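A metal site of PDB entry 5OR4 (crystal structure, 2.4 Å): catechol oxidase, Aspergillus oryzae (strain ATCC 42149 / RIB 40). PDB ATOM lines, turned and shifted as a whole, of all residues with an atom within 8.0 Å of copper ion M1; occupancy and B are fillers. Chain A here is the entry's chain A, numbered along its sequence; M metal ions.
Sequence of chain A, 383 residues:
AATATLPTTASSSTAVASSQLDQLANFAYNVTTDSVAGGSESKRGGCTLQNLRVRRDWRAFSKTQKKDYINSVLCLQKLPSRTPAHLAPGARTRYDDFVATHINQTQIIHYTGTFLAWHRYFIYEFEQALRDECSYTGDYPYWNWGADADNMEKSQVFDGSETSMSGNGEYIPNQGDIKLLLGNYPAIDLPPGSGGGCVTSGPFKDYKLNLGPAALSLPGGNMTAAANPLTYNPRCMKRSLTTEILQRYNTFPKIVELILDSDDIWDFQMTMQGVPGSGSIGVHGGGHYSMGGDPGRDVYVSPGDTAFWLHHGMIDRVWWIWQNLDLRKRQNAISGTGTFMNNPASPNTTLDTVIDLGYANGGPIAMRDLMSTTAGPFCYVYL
Copper ion M1 is bound by NE2 of His 119 (2.1 Å). NE2 of His 102 binds copper ion M1. Copper ion M1 is bound by a ring nitrogen (NE2) of His 110, 2.2 Å away. Copper ion M1 has three donor atoms within binding distance.
Residues that only touch copper ion M1: Ile 109 (3.7 Å). Within 4 Å of copper ion M1: His 102, Ile 109, His 110 and His 119.
ND1 of His 102 sits at hydrogen-bond distance from O of Tyr 300, 2.6 Å away. OG1 of Thr 106 lies within hydrogen-bond range of O of His 102 (2.5 Å). ND1 of His 119 is in hydrogen-bond range of O of Phe 115 (2.8 Å). ND1 of His 110 lies within hydrogen-bond range of O of Thr 106 (3.0 Å).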
ATOM      1  N   HIS A 102      14.154  14.194   9.311  1.00  0.00           N
ATOM      2  CA  HIS A 102      13.891  14.531   7.918  1.00  0.00           C
ATOM      3  C   HIS A 102      15.175  14.487   7.092  1.00  0.00           C
ATOM      4  O   HIS A 102      15.179  13.968   5.974  1.00  0.00           O
ATOM      5  CB  HIS A 102      13.242  15.916   7.822  1.00  0.00           C
ATOM      6  CG  HIS A 102      12.700  16.241   6.470  1.00  0.00           C
ATOM      7  ND1 HIS A 102      13.439  16.893   5.502  1.00  0.00           N
ATOM      8  CD2 HIS A 102      11.482  16.008   5.903  1.00  0.00           C
ATOM      9  CE1 HIS A 102      12.710  17.047   4.412  1.00  0.00           C
ATOM     10  NE2 HIS A 102      11.519  16.514   4.631  1.00  0.00           N
ATOM     11  N   ILE A 103      16.265  15.041   7.627  1.00  0.00           N
ATOM     12  CA  ILE A 103      17.562  14.936   6.955  1.00  0.00           C
ATOM     13  C   ILE A 103      17.946  13.470   6.779  1.00  0.00           C
ATOM     14  O   ILE A 103      18.339  13.037   5.695  1.00  0.00           O
ATOM     15  CB  ILE A 103      18.635  15.696   7.742  1.00  0.00           C
ATOM     16  CG1 ILE A 103      18.273  17.180   7.867  1.00  0.00           C
ATOM     17  CG2 ILE A 103      20.001  15.529   7.086  1.00  0.00           C
ATOM     18  CD1 ILE A 103      19.204  17.946   8.786  1.00  0.00           C
ATOM     19  N   GLN A 105      16.178  10.836   6.535  1.00  0.00           N
ATOM     20  CA  GLN A 105      15.293  10.015   5.708  1.00  0.00           C
ATOM     21  C   GLN A 105      14.922  10.669   4.382  1.00  0.00           C
ATOM     22  O   GLN A 105      14.010  10.192   3.716  1.00  0.00           O
ATOM     23  CB  GLN A 105      14.016   9.688   6.471  1.00  0.00           C
ATOM     24  CG  GLN A 105      14.215   8.884   7.740  1.00  0.00           C
ATOM     25  CD  GLN A 105      12.911   8.304   8.256  1.00  0.00           C
ATOM     26  OE1 GLN A 105      12.226   7.574   7.545  1.00  0.00           O
ATOM     27  NE2 GLN A 105      12.560   8.642   9.492  1.00  0.00           N
ATOM     28  N   THR A 106      15.611  11.742   3.981  1.00  0.00           N
ATOM     29  CA  THR A 106      15.187  12.501   2.813  1.00  0.00           C
ATOM     30  C   THR A 106      15.170  11.643   1.548  1.00  0.00           C
ATOM     31  O   THR A 106      14.264  11.775   0.716  1.00  0.00           O
ATOM     32  CB  THR A 106      16.085  13.725   2.620  1.00  0.00           C
ATOM     33  OG1 THR A 106      15.800  14.695   3.634  1.00  0.00           O
ATOM     34  CG2 THR A 106      15.868  14.365   1.254  1.00  0.00           C
ATOM     35  N   ILE A 109      11.849   9.399   1.234  1.00  0.00           N
ATOM     36  CA  ILE A 109      10.551  10.006   1.515  1.00  0.00           C
ATOM     37  C   ILE A 109      10.134  10.999   0.429  1.00  0.00           C
ATOM     38  O   ILE A 109       9.028  11.537   0.477  1.00  0.00           O
ATOM     39  CB  ILE A 109      10.540  10.705   2.887  1.00  0.00           C
ATOM     40  CG1 ILE A 109      11.476  11.922   2.891  1.00  0.00           C
ATOM     41  CG2 ILE A 109      10.882   9.726   4.007  1.00  0.00           C
ATOM     42  CD1 ILE A 109      11.505  12.660   4.208  1.00  0.00           C
ATOM     43  N   HIS A 110      11.007  11.245  -0.537  1.00  0.00           N
ATOM     44  CA  HIS A 110      10.689  12.109  -1.670  1.00  0.00           C
ATOM     45  C   HIS A 110      10.817  11.313  -2.956  1.00  0.00           C
ATOM     46  O   HIS A 110      11.782  10.574  -3.138  1.00  0.00           O
ATOM     47  CB  HIS A 110      11.598  13.349  -1.703  1.00  0.00           C
ATOM     48  CG  HIS A 110      11.511  14.194  -0.463  1.00  0.00           C
ATOM     49  ND1 HIS A 110      12.485  14.167   0.513  1.00  0.00           N
ATOM     50  CD2 HIS A 110      10.591  15.085  -0.049  1.00  0.00           C
ATOM     51  CE1 HIS A 110      12.152  14.999   1.481  1.00  0.00           C
ATOM     52  NE2 HIS A 110      11.005  15.578   1.163  1.00  0.00           N
ATOM     53  N   PHE A 115       5.757   9.239  -0.074  1.00  0.00           N
ATOM     54  CA  PHE A 115       5.966  10.674   0.025  1.00  0.00           C
ATOM     55  C   PHE A 115       4.777  11.387   0.657  1.00  0.00           C
ATOM     56  O   PHE A 115       4.927  12.146   1.621  1.00  0.00           O
ATOM     57  CB  PHE A 115       6.264  11.267  -1.356  1.00  0.00           C
ATOM     58  CG  PHE A 115       6.094  12.758  -1.418  1.00  0.00           C
ATOM     59  CD1 PHE A 115       6.953  13.598  -0.731  1.00  0.00           C
ATOM     60  CD2 PHE A 115       5.065  13.324  -2.164  1.00  0.00           C
ATOM     61  CE1 PHE A 115       6.793  14.971  -0.782  1.00  0.00           C
ATOM     62  CE2 PHE A 115       4.910  14.692  -2.220  1.00  0.00           C
ATOM     63  CZ  PHE A 115       5.774  15.519  -1.532  1.00  0.00           C
ATOM     64  N   TRP A 118       3.978   9.862   4.311  1.00  0.00           N
ATOM     65  CA  TRP A 118       4.987  10.164   5.312  1.00  0.00           C
ATOM     66  C   TRP A 118       4.837  11.587   5.844  1.00  0.00           C
ATOM     67  O   TRP A 118       4.986  11.832   7.043  1.00  0.00           O
ATOM     68  CB  TRP A 118       6.385   9.951   4.742  1.00  0.00           C
ATOM     69  CG  TRP A 118       7.483  10.007   5.760  1.00  0.00           C
ATOM     70  CD1 TRP A 118       8.038   8.950   6.423  1.00  0.00           C
ATOM     71  CD2 TRP A 118       8.170  11.175   6.229  1.00  0.00           C
ATOM     72  NE1 TRP A 118       9.025   9.386   7.270  1.00  0.00           N
ATOM     73  CE2 TRP A 118       9.119  10.746   7.179  1.00  0.00           C
ATOM     74  CE3 TRP A 118       8.061  12.540   5.948  1.00  0.00           C
ATOM     75  CZ2 TRP A 118       9.957  11.636   7.842  1.00  0.00           C
ATOM     76  CZ3 TRP A 118       8.896  13.421   6.601  1.00  0.00           C
ATOM     77  CH2 TRP A 118       9.834  12.971   7.542  1.00  0.00           C
ATOM     78  N   HIS A 119       4.548  12.545   4.952  1.00  0.00           N
ATOM     79  CA  HIS A 119       4.437  13.933   5.382  1.00  0.00           C
ATOM     80  C   HIS A 119       3.120  14.201   6.089  1.00  0.00           C
ATOM     81  O   HIS A 119       3.069  15.078   6.964  1.00  0.00           O
ATOM     82  CB  HIS A 119       4.605  14.855   4.178  1.00  0.00           C
ATOM     83  CG  HIS A 119       6.017  14.954   3.684  1.00  0.00           C
ATOM     84  ND1 HIS A 119       6.551  14.055   2.786  1.00  0.00           N
ATOM     85  CD2 HIS A 119       7.012  15.824   3.986  1.00  0.00           C
ATOM     86  CE1 HIS A 119       7.812  14.377   2.546  1.00  0.00           C
ATOM     87  NE2 HIS A 119       8.116  15.448   3.259  1.00  0.00           N
ATOM     88  N   PHE A 122       4.095  13.109   9.347  1.00  0.00           N
ATOM     89  CA  PHE A 122       5.119  13.988   9.892  1.00  0.00           C
ATOM     90  C   PHE A 122       4.505  15.211  10.567  1.00  0.00           C
ATOM     91  O   PHE A 122       4.835  15.528  11.718  1.00  0.00           O
ATOM     92  CB  PHE A 122       6.072  14.423   8.769  1.00  0.00           C
ATOM     93  CG  PHE A 122       7.329  15.087   9.251  1.00  0.00           C
ATOM     94  CD1 PHE A 122       8.011  14.604  10.358  1.00  0.00           C
ATOM     95  CD2 PHE A 122       7.850  16.187   8.585  1.00  0.00           C
ATOM     96  CE1 PHE A 122       9.170  15.211  10.798  1.00  0.00           C
ATOM     97  CE2 PHE A 122       9.010  16.800   9.018  1.00  0.00           C
ATOM     98  CZ  PHE A 122       9.670  16.316  10.121  1.00  0.00           C
ATOM     99  N   GLN A 273       5.157  17.110  -7.293  1.00  0.00           N
ATOM    100  CA  GLN A 273       6.560  17.318  -6.959  1.00  0.00           C
ATOM    101  C   GLN A 273       7.381  17.875  -8.102  1.00  0.00           C
ATOM    102  O   GLN A 273       8.448  18.469  -7.858  1.00  0.00           O
ATOM    103  CB  GLN A 273       7.192  16.009  -6.487  1.00  0.00           C
ATOM    104  CG  GLN A 273       6.576  15.440  -5.219  1.00  0.00           C
ATOM    105  CD  GLN A 273       7.083  14.040  -4.911  1.00  0.00           C
ATOM    106  OE1 GLN A 273       8.122  13.868  -4.276  1.00  0.00           O
ATOM    107  NE2 GLN A 273       6.338  13.035  -5.365  1.00  0.00           N
ATOM    108  N   HIS A 284       4.603  21.649  -5.018  1.00  0.00           N
ATOM    109  CA  HIS A 284       5.435  21.321  -3.864  1.00  0.00           C
ATOM    110  C   HIS A 284       6.795  22.018  -3.969  1.00  0.00           C
ATOM    111  O   HIS A 284       7.254  22.651  -3.010  1.00  0.00           O
ATOM    112  CB  HIS A 284       5.612  19.808  -3.753  1.00  0.00           C
ATOM    113  CG  HIS A 284       6.541  19.390  -2.652  1.00  0.00           C
ATOM    114  ND1 HIS A 284       7.764  18.796  -2.900  1.00  0.00           N
ATOM    115  CD2 HIS A 284       6.427  19.474  -1.303  1.00  0.00           C
ATOM    116  CE1 HIS A 284       8.365  18.546  -1.751  1.00  0.00           C
ATOM    117  NE2 HIS A 284       7.573  18.943  -0.764  1.00  0.00           N
ATOM    118  N   HIS A 288       8.394  25.486  -1.716  1.00  0.00           N
ATOM    119  CA  HIS A 288       9.643  25.457  -0.955  1.00  0.00           C
ATOM    120  C   HIS A 288      10.593  26.557  -1.397  1.00  0.00           C
ATOM    121  O   HIS A 288      11.109  27.312  -0.566  1.00  0.00           O
ATOM    122  CB  HIS A 288      10.318  24.090  -1.110  1.00  0.00           C
ATOM    123  CG  HIS A 288       9.759  23.035  -0.201  1.00  0.00           C
ATOM    124  ND1 HIS A 288      10.084  22.960   1.137  1.00  0.00           N
ATOM    125  CD2 HIS A 288       8.908  22.015  -0.440  1.00  0.00           C
ATOM    126  CE1 HIS A 288       9.453  21.934   1.678  1.00  0.00           C
ATOM    127  NE2 HIS A 288       8.731  21.347   0.750  1.00  0.00           N
ATOM    128  N   VAL A 299      16.835  20.588   0.280  1.00  0.00           N
ATOM    129  CA  VAL A 299      15.800  19.564   0.232  1.00  0.00           C
ATOM    130  C   VAL A 299      15.791  18.752   1.523  1.00  0.00           C
ATOM    131  O   VAL A 299      14.724  18.285   1.969  1.00  0.00           O
ATOM    132  CB  VAL A 299      16.008  18.675  -1.011  1.00  0.00           C
ATOM    133  CG1 VAL A 299      15.222  17.376  -0.909  1.00  0.00           C
ATOM    134  CG2 VAL A 299      15.623  19.437  -2.271  1.00  0.00           C
ATOM    135  N   TYR A 300      16.940  18.587   2.178  1.00  0.00           N
ATOM    136  CA  TYR A 300      17.010  17.797   3.402  1.00  0.00           C
ATOM    137  C   TYR A 300      16.543  18.607   4.618  1.00  0.00           C
ATOM    138  O   TYR A 300      15.755  18.100   5.428  1.00  0.00           O
ATOM    139  CB  TYR A 300      18.440  17.303   3.638  1.00  0.00           C
ATOM    140  CG  TYR A 300      19.036  16.401   2.572  1.00  0.00           C
ATOM    141  CD1 TYR A 300      19.392  16.910   1.327  1.00  0.00           C
ATOM    142  CD2 TYR A 300      19.285  15.063   2.826  1.00  0.00           C
ATOM    143  CE1 TYR A 300      19.951  16.097   0.361  1.00  0.00           C
ATOM    144  CE2 TYR A 300      19.843  14.243   1.868  1.00  0.00           C
ATOM    145  CZ  TYR A 300      20.174  14.766   0.635  1.00  0.00           C
ATOM    146  OH  TYR A 300      20.740  13.950  -0.319  1.00  0.00           O
ATOM    147  N   SER A 302      14.843  21.372   4.862  1.00  0.00           N
ATOM    148  CA  SER A 302      13.732  22.306   4.653  1.00  0.00           C
ATOM    149  C   SER A 302      12.778  22.451   5.836  1.00  0.00           C
ATOM    150  O   SER A 302      12.242  23.568   6.011  1.00  0.00           O
ATOM    151  CB  SER A 302      12.944  21.906   3.393  1.00  0.00           C
ATOM    152  OG  SER A 302      12.403  20.611   3.498  1.00  0.00           O
ATOM    153  N   PRO A 303      12.511  21.440   6.680  1.00  0.00           N
ATOM    154  CA  PRO A 303      11.698  21.687   7.884  1.00  0.00           C
ATOM    155  C   PRO A 303      12.300  22.710   8.827  1.00  0.00           C
ATOM    156  O   PRO A 303      11.595  23.184   9.731  1.00  0.00           O
ATOM    157  CB  PRO A 303      11.609  20.304   8.541  1.00  0.00           C
ATOM    158  CG  PRO A 303      11.744  19.369   7.416  1.00  0.00           C
ATOM    159  CD  PRO A 303      12.746  19.991   6.490  1.00  0.00           C
ATOM    160  N   PHE A 308       7.481  25.637   6.763  1.00  0.00           N
ATOM    161  CA  PHE A 308       7.370  24.282   6.241  1.00  0.00           C
ATOM    162  C   PHE A 308       6.056  23.632   6.657  1.00  0.00           C
ATOM    163  O   PHE A 308       5.409  22.944   5.849  1.00  0.00           O
ATOM    164  CB  PHE A 308       8.563  23.450   6.721  1.00  0.00           C
ATOM    165  CG  PHE A 308       8.460  21.975   6.450  1.00  0.00           C
ATOM    166  CD1 PHE A 308       7.857  21.124   7.361  1.00  0.00           C
ATOM    167  CD2 PHE A 308       9.012  21.435   5.305  1.00  0.00           C
ATOM    168  CE1 PHE A 308       7.760  19.769   7.113  1.00  0.00           C
ATOM    169  CE2 PHE A 308       8.929  20.077   5.056  1.00  0.00           C
ATOM    170  CZ  PHE A 308       8.308  19.250   5.959  1.00  0.00           C
ATOM    171  N   HIS A 312       3.136  22.323   4.217  1.00  0.00           N
ATOM    172  CA  HIS A 312       2.717  20.939   4.074  1.00  0.00           C
ATOM    173  C   HIS A 312       1.316  20.675   4.616  1.00  0.00           C
ATOM    174  O   HIS A 312       0.771  19.596   4.368  1.00  0.00           O
ATOM    175  CB  HIS A 312       3.728  20.023   4.763  1.00  0.00           C
ATOM    176  CG  HIS A 312       4.765  19.483   3.831  1.00  0.00           C
ATOM    177  ND1 HIS A 312       4.529  18.430   2.987  1.00  0.00           N
ATOM    178  CD2 HIS A 312       6.033  19.885   3.602  1.00  0.00           C
ATOM    179  CE1 HIS A 312       5.614  18.193   2.270  1.00  0.00           C
ATOM    180  NE2 HIS A 312       6.545  19.052   2.625  1.00  0.00           N
HETATM  181 CU    CU M   1      10.121  15.973   3.141  1.00  0.00          CU
HETATM  182 CU    CU M   2       7.867  19.607   1.181  1.00  0.00          CU
